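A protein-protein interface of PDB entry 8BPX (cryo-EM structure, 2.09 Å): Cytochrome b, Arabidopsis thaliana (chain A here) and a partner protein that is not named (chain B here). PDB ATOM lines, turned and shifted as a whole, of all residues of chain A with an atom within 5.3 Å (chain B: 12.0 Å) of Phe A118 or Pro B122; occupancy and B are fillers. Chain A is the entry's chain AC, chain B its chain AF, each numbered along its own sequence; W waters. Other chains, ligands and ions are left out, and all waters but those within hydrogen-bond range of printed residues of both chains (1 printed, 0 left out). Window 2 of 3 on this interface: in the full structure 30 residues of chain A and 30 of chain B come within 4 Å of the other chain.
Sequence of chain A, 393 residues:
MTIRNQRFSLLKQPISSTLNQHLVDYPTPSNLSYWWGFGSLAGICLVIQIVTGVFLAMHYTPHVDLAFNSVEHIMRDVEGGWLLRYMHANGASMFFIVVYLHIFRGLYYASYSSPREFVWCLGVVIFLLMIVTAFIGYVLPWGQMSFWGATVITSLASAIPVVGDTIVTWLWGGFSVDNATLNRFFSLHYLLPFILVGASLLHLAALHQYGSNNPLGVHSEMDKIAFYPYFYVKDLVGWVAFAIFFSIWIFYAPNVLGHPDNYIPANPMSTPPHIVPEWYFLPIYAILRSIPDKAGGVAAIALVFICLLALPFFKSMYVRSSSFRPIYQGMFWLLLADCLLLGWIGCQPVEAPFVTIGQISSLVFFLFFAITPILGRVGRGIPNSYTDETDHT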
ATOM      1  N   PRO A 115     -11.111  11.074 -31.068  1.00  0.00           N
ATOM      2  CA  PRO A 115     -11.771  12.337 -30.729  1.00  0.00           C
ATOM      3  C   PRO A 115     -10.882  13.313 -29.961  1.00  0.00           C
ATOM      4  O   PRO A 115     -11.398  14.179 -29.269  1.00  0.00           O
ATOM      5  CB  PRO A 115     -12.938  11.857 -29.865  1.00  0.00           C
ATOM      6  CG  PRO A 115     -12.339  10.687 -29.090  1.00  0.00           C
ATOM      7  CD  PRO A 115     -11.229  10.109 -29.962  1.00  0.00           C
ATOM      8  N   ARG A 116      -9.556  13.217 -30.057  1.00  0.00           N
ATOM      9  CA  ARG A 116      -8.659  13.981 -29.198  1.00  0.00           C
ATOM     10  C   ARG A 116      -8.010  15.163 -29.914  1.00  0.00           C
ATOM     11  O   ARG A 116      -6.920  15.597 -29.524  1.00  0.00           O
ATOM     12  CB  ARG A 116      -7.593  13.057 -28.608  1.00  0.00           C
ATOM     13  CG  ARG A 116      -8.123  12.121 -27.539  1.00  0.00           C
ATOM     14  CD  ARG A 116      -7.086  11.104 -27.100  1.00  0.00           C
ATOM     15  NE  ARG A 116      -7.694  10.026 -26.333  1.00  0.00           N
ATOM     16  CZ  ARG A 116      -8.238   8.939 -26.862  1.00  0.00           C
ATOM     17  NH1 ARG A 116      -8.243   8.733 -28.169  1.00  0.00           N
ATOM     18  NH2 ARG A 116      -8.795   8.040 -26.059  1.00  0.00           N
ATOM     19  N   GLU A 117      -8.667  15.703 -30.945  1.00  0.00           N
ATOM     20  CA  GLU A 117      -8.085  16.797 -31.721  1.00  0.00           C
ATOM     21  C   GLU A 117      -7.867  18.045 -30.866  1.00  0.00           C
ATOM     22  O   GLU A 117      -6.833  18.717 -30.982  1.00  0.00           O
ATOM     23  CB  GLU A 117      -8.983  17.122 -32.916  1.00  0.00           C
ATOM     24  CG  GLU A 117      -9.257  15.942 -33.840  1.00  0.00           C
ATOM     25  CD  GLU A 117     -10.636  15.338 -33.633  1.00  0.00           C
ATOM     26  OE1 GLU A 117     -10.982  15.027 -32.478  1.00  0.00           O
ATOM     27  OE2 GLU A 117     -11.370  15.165 -34.627  1.00  0.00           O
ATOM     28  N   PHE A 118      -8.833  18.372 -30.006  1.00  0.00           N
ATOM     29  CA  PHE A 118      -8.720  19.561 -29.167  1.00  0.00           C
ATOM     30  C   PHE A 118      -7.555  19.441 -28.190  1.00  0.00           C
ATOM     31  O   PHE A 118      -6.882  20.434 -27.888  1.00  0.00           O
ATOM     32  CB  PHE A 118     -10.038  19.797 -28.429  1.00  0.00           C
ATOM     33  CG  PHE A 118     -10.163  21.163 -27.817  1.00  0.00           C
ATOM     34  CD1 PHE A 118      -9.848  22.297 -28.545  1.00  0.00           C
ATOM     35  CD2 PHE A 118     -10.609  21.313 -26.517  1.00  0.00           C
ATOM     36  CE1 PHE A 118      -9.969  23.557 -27.980  1.00  0.00           C
ATOM     37  CE2 PHE A 118     -10.734  22.573 -25.949  1.00  0.00           C
ATOM     38  CZ  PHE A 118     -10.410  23.692 -26.683  1.00  0.00           C
ATOM     39  N   VAL A 119      -7.299  18.226 -27.691  1.00  0.00           N
ATOM     40  CA  VAL A 119      -6.140  17.993 -26.834  1.00  0.00           C
ATOM     41  C   VAL A 119      -4.860  18.376 -27.565  1.00  0.00           C
ATOM     42  O   VAL A 119      -4.007  19.099 -27.036  1.00  0.00           O
ATOM     43  CB  VAL A 119      -6.105  16.524 -26.371  1.00  0.00           C
ATOM     44  CG1 VAL A 119      -5.137  16.339 -25.212  1.00  0.00           C
ATOM     45  CG2 VAL A 119      -7.500  16.041 -25.998  1.00  0.00           C
ATOM     46  N   TRP A 120      -4.726  17.922 -28.812  1.00  0.00           N
ATOM     47  CA  TRP A 120      -3.533  18.226 -29.592  1.00  0.00           C
ATOM     48  C   TRP A 120      -3.406  19.719 -29.878  1.00  0.00           C
ATOM     49  O   TRP A 120      -2.303  20.273 -29.821  1.00  0.00           O
ATOM     50  CB  TRP A 120      -3.544  17.428 -30.892  1.00  0.00           C
ATOM     51  CG  TRP A 120      -2.303  17.600 -31.681  1.00  0.00           C
ATOM     52  CD1 TRP A 120      -2.112  18.456 -32.720  1.00  0.00           C
ATOM     53  CD2 TRP A 120      -1.065  16.915 -31.491  1.00  0.00           C
ATOM     54  NE1 TRP A 120      -0.835  18.339 -33.199  1.00  0.00           N
ATOM     55  CE2 TRP A 120      -0.170  17.399 -32.462  1.00  0.00           C
ATOM     56  CE3 TRP A 120      -0.627  15.931 -30.602  1.00  0.00           C
ATOM     57  CZ2 TRP A 120       1.138  16.937 -32.566  1.00  0.00           C
ATOM     58  CZ3 TRP A 120       0.669  15.475 -30.706  1.00  0.00           C
ATOM     59  CH2 TRP A 120       1.538  15.978 -31.683  1.00  0.00           C
ATOM     60  N   CYS A 121      -4.517  20.382 -30.206  1.00  0.00           N
ATOM     61  CA  CYS A 121      -4.455  21.815 -30.490  1.00  0.00           C
ATOM     62  C   CYS A 121      -4.053  22.616 -29.254  1.00  0.00           C
ATOM     63  O   CYS A 121      -3.229  23.539 -29.339  1.00  0.00           O
ATOM     64  CB  CYS A 121      -5.794  22.305 -31.044  1.00  0.00           C
ATOM     65  SG  CYS A 121      -6.312  21.489 -32.566  1.00  0.00           S
ATOM     66  N   LEU A 122      -4.614  22.270 -28.094  1.00  0.00           N
ATOM     67  CA  LEU A 122      -4.200  22.923 -26.857  1.00  0.00           C
ATOM     68  C   LEU A 122      -2.727  22.656 -26.569  1.00  0.00           C
ATOM     69  O   LEU A 122      -2.012  23.542 -26.089  1.00  0.00           O
ATOM     70  CB  LEU A 122      -5.078  22.462 -25.696  1.00  0.00           C
ATOM     71  CG  LEU A 122      -6.502  23.027 -25.667  1.00  0.00           C
ATOM     72  CD1 LEU A 122      -7.371  22.269 -24.673  1.00  0.00           C
ATOM     73  CD2 LEU A 122      -6.503  24.526 -25.359  1.00  0.00           C
ATOM     74  N   GLY A 123      -2.250  21.446 -26.874  1.00  0.00           N
ATOM     75  CA  GLY A 123      -0.832  21.164 -26.725  1.00  0.00           C
ATOM     76  C   GLY A 123       0.041  22.031 -27.614  1.00  0.00           C
ATOM     77  O   GLY A 123       1.105  22.489 -27.199  1.00  0.00           O
ATOM     78  N   ALA A 206      -9.542  18.641 -21.455  1.00  0.00           N
ATOM     79  CA  ALA A 206      -9.863  18.136 -22.784  1.00  0.00           C
ATOM     80  C   ALA A 206      -9.500  16.662 -22.907  1.00  0.00           C
ATOM     81  O   ALA A 206     -10.252  15.880 -23.494  1.00  0.00           O
ATOM     82  CB  ALA A 206      -9.153  18.964 -23.855  1.00  0.00           C
ATOM     83  N   GLN A 209     -12.047  14.468 -21.254  1.00  0.00           N
ATOM     84  CA  GLN A 209     -13.321  14.290 -21.947  1.00  0.00           C
ATOM     85  C   GLN A 209     -13.489  12.851 -22.455  1.00  0.00           C
ATOM     86  O   GLN A 209     -14.557  12.250 -22.296  1.00  0.00           O
ATOM     87  CB  GLN A 209     -13.473  15.269 -23.110  1.00  0.00           C
ATOM     88  CG  GLN A 209     -14.715  14.973 -23.949  1.00  0.00           C
ATOM     89  CD  GLN A 209     -15.067  16.070 -24.930  1.00  0.00           C
ATOM     90  OE1 GLN A 209     -16.171  16.100 -25.471  1.00  0.00           O
ATOM     91  NE2 GLN A 209     -14.131  16.978 -25.164  1.00  0.00           N
ATOM     92  N   TYR A 210     -12.441  12.276 -23.055  1.00  0.00           N
ATOM     93  CA  TYR A 210     -12.525  10.938 -23.629  1.00  0.00           C
ATOM     94  C   TYR A 210     -11.586   9.921 -22.995  1.00  0.00           C
ATOM     95  O   TYR A 210     -11.714   8.727 -23.285  1.00  0.00           O
ATOM     96  CB  TYR A 210     -12.242  10.983 -25.140  1.00  0.00           C
ATOM     97  CG  TYR A 210     -13.245  11.801 -25.911  1.00  0.00           C
ATOM     98  CD1 TYR A 210     -14.539  11.343 -26.105  1.00  0.00           C
ATOM     99  CD2 TYR A 210     -12.901  13.038 -26.433  1.00  0.00           C
ATOM    100  CE1 TYR A 210     -15.457  12.089 -26.804  1.00  0.00           C
ATOM    101  CE2 TYR A 210     -13.812  13.792 -27.132  1.00  0.00           C
ATOM    102  CZ  TYR A 210     -15.090  13.312 -27.316  1.00  0.00           C
ATOM    103  OH  TYR A 210     -16.004  14.058 -28.016  1.00  0.00           O
ATOM    104  N   LEU B  42     -15.244   5.557 -30.796  1.00  0.00           N
ATOM    105  CA  LEU B  42     -14.897   6.971 -30.444  1.00  0.00           C
ATOM    106  C   LEU B  42     -14.232   7.725 -31.615  1.00  0.00           C
ATOM    107  O   LEU B  42     -14.317   8.919 -31.591  1.00  0.00           O
ATOM    108  CB  LEU B  42     -14.130   7.071 -29.102  1.00  0.00           C
ATOM    109  CG  LEU B  42     -14.756   6.366 -27.906  1.00  0.00           C
ATOM    110  CD1 LEU B  42     -13.865   6.451 -26.675  1.00  0.00           C
ATOM    111  CD2 LEU B  42     -16.147   6.887 -27.607  1.00  0.00           C
ATOM    112  N   TYR B  43     -13.649   7.044 -32.613  1.00  0.00           N
ATOM    113  CA  TYR B  43     -13.052   7.695 -33.794  1.00  0.00           C
ATOM    114  C   TYR B  43     -14.104   8.333 -34.711  1.00  0.00           C
ATOM    115  O   TYR B  43     -13.871   9.367 -35.186  1.00  0.00           O
ATOM    116  CB  TYR B  43     -12.121   6.744 -34.577  1.00  0.00           C
ATOM    117  CG  TYR B  43     -11.458   7.364 -35.771  1.00  0.00           C
ATOM    118  CD1 TYR B  43     -12.092   7.402 -36.996  1.00  0.00           C
ATOM    119  CD2 TYR B  43     -10.205   7.932 -35.664  1.00  0.00           C
ATOM    120  CE1 TYR B  43     -11.492   7.989 -38.091  1.00  0.00           C
ATOM    121  CE2 TYR B  43      -9.599   8.540 -36.748  1.00  0.00           C
ATOM    122  CZ  TYR B  43     -10.240   8.559 -37.969  1.00  0.00           C
ATOM    123  OH  TYR B  43      -9.648   9.132 -39.055  1.00  0.00           O
ATOM    124  N   LEU B  45     -18.546   8.537 -35.611  1.00  0.00           N
ATOM    125  CA  LEU B  45     -19.928   8.236 -35.253  1.00  0.00           C
ATOM    126  C   LEU B  45     -20.521   7.150 -36.146  1.00  0.00           C
ATOM    127  O   LEU B  45     -21.388   6.392 -35.698  1.00  0.00           O
ATOM    128  CB  LEU B  45     -20.771   9.512 -35.316  1.00  0.00           C
ATOM    129  CG  LEU B  45     -20.911  10.371 -34.051  1.00  0.00           C
ATOM    130  CD1 LEU B  45     -21.773   9.697 -33.001  1.00  0.00           C
ATOM    131  CD2 LEU B  45     -19.560  10.730 -33.456  1.00  0.00           C
ATOM    132  N   GLN B 118     -24.873  13.102 -34.647  1.00  0.00           N
ATOM    133  CA  GLN B 118     -23.819  14.089 -34.795  1.00  0.00           C
ATOM    134  C   GLN B 118     -22.783  13.895 -33.705  1.00  0.00           C
ATOM    135  O   GLN B 118     -23.082  13.393 -32.621  1.00  0.00           O
ATOM    136  CB  GLN B 118     -24.367  15.519 -34.743  1.00  0.00           C
ATOM    137  CG  GLN B 118     -24.758  16.075 -36.087  1.00  0.00           C
ATOM    138  CD  GLN B 118     -25.359  17.460 -35.987  1.00  0.00           C
ATOM    139  OE1 GLN B 118     -26.310  17.684 -35.241  1.00  0.00           O
ATOM    140  NE2 GLN B 118     -24.803  18.401 -36.738  1.00  0.00           N
ATOM    141  N   ARG B 119     -21.557  14.298 -34.010  1.00  0.00           N
ATOM    142  CA  ARG B 119     -20.499  14.314 -33.015  1.00  0.00           C
ATOM    143  C   ARG B 119     -20.635  15.544 -32.127  1.00  0.00           C
ATOM    144  O   ARG B 119     -20.945  16.638 -32.602  1.00  0.00           O
ATOM    145  CB  ARG B 119     -19.133  14.311 -33.692  1.00  0.00           C
ATOM    146  CG  ARG B 119     -18.008  13.986 -32.753  1.00  0.00           C
ATOM    147  CD  ARG B 119     -16.798  14.821 -33.050  1.00  0.00           C
ATOM    148  NE  ARG B 119     -15.871  14.821 -31.928  1.00  0.00           N
ATOM    149  CZ  ARG B 119     -14.556  14.719 -32.048  1.00  0.00           C
ATOM    150  NH1 ARG B 119     -13.981  14.581 -33.232  1.00  0.00           N
ATOM    151  NH2 ARG B 119     -13.802  14.757 -30.956  1.00  0.00           N
ATOM    152  N   THR B 120     -20.404  15.356 -30.832  1.00  0.00           N
ATOM    153  CA  THR B 120     -20.393  16.484 -29.910  1.00  0.00           C
ATOM    154  C   THR B 120     -19.159  17.352 -30.137  1.00  0.00           C
ATOM    155  O   THR B 120     -18.102  16.873 -30.555  1.00  0.00           O
ATOM    156  CB  THR B 120     -20.434  15.997 -28.461  1.00  0.00           C
ATOM    157  OG1 THR B 120     -19.301  15.160 -28.200  1.00  0.00           O
ATOM    158  CG2 THR B 120     -21.702  15.211 -28.197  1.00  0.00           C
ATOM    159  N   ILE B 121     -19.305  18.646 -29.872  1.00  0.00           N
ATOM    160  CA  ILE B 121     -18.190  19.585 -29.975  1.00  0.00           C
ATOM    161  C   ILE B 121     -17.402  19.557 -28.669  1.00  0.00           C
ATOM    162  O   ILE B 121     -17.938  19.922 -27.615  1.00  0.00           O
ATOM    163  CB  ILE B 121     -18.675  21.008 -30.298  1.00  0.00           C
ATOM    164  CG1 ILE B 121     -19.356  21.050 -31.664  1.00  0.00           C
ATOM    165  CG2 ILE B 121     -17.511  21.989 -30.253  1.00  0.00           C
ATOM    166  CD1 ILE B 121     -20.222  22.263 -31.880  1.00  0.00           C
ATOM    167  N   PRO B 122     -16.128  19.143 -28.694  1.00  0.00           N
ATOM    168  CA  PRO B 122     -15.284  19.022 -27.502  1.00  0.00           C
ATOM    169  C   PRO B 122     -14.722  20.354 -27.032  1.00  0.00           C
ATOM    170  O   PRO B 122     -13.501  20.497 -27.020  1.00  0.00           O
ATOM    171  CB  PRO B 122     -14.161  18.102 -27.972  1.00  0.00           C
ATOM    172  CG  PRO B 122     -14.032  18.403 -29.415  1.00  0.00           C
ATOM    173  CD  PRO B 122     -15.409  18.747 -29.917  1.00  0.00           C
HETATM  174  O   HOH W   1     -18.470  14.009 -25.817  1.00  0.00           O
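The guanidinium group (NH2) of Arg B119 sits at hydrogen-bond distance from the backbone carbonyl oxygen (O) of Pro A115 (3.0 Å). OE2 of Glu A117 is in salt-bridge range of NH1 of Arg B119, 3.0 Å away. OH of Tyr A210 lies within hydrogen-bond range of OG1 of Thr B120.
Of chain B, only Pro B122 comes within 4 Å of Phe A118. Of chain A, only Phe A118 (3.0 Å) and Gln A209 (3.0 Å) come within 4 Å of Pro B122. Glu A117 touches just one residue of chain B: Arg B119 (3.0 Å). No residue of chain B comes within 4 Å of Cys A121. No residue of chain B comes within 4 Å of Leu A122. No residue of chain B comes within 4 Å of Ala A206. Of the printed residues of chain B, Pro A115 touches Leu B42 and Arg B119. Of the printed residues of chain A, Thr B120 touches Tyr A210 (3.5 Å). Of the printed residues of chain A, Leu B42 touches Pro A115. Printed residues of chain B within 4 Å of Gln A209: Pro B122 (3.0 Å). Arg A116 touches none of the printed residues of chain B. Gln B118 touches none of the printed residues of chain A. The nearest printed residue of chain A that does not touch Thr B120 is Gln A209 (4.3 Å).
Water W1 lies within hydrogen-bond range of OG1 of Thr B120, OE1 of Gln A209 and OH of Tyr A210.
Of the 8 printed residues of chain B, 4 touch a printed residue of chain A. Printed residues of chain B that touch a printed residue of chain A: Leu B42, Arg B119, Thr B120 and Pro B122. Of the 12 printed residues of chain A, 5 touch a printed residue of chain B. Among the printed residues, 7 pairs touch across the chains. Among the printed residues, Asp or Glu carboxylates within 4 Å of a Lys or Arg side-chain nitrogen of the other chain: Glu A117 with Arg B119 (3.0 Å).
Among the printed residues, pairs that only touch across the chains: Gln A209 with Pro B122, Phe A118 with Pro B122, Pro A115 with Leu B42 and Tyr A210 with Arg B119.
SG of Cys A121 is in hydrogen-bond range of O of Glu A117, 3.2 Å away. OE1 of Gln A209 lies within hydrogen-bond range of OH of Tyr A210 (3.3 Å).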
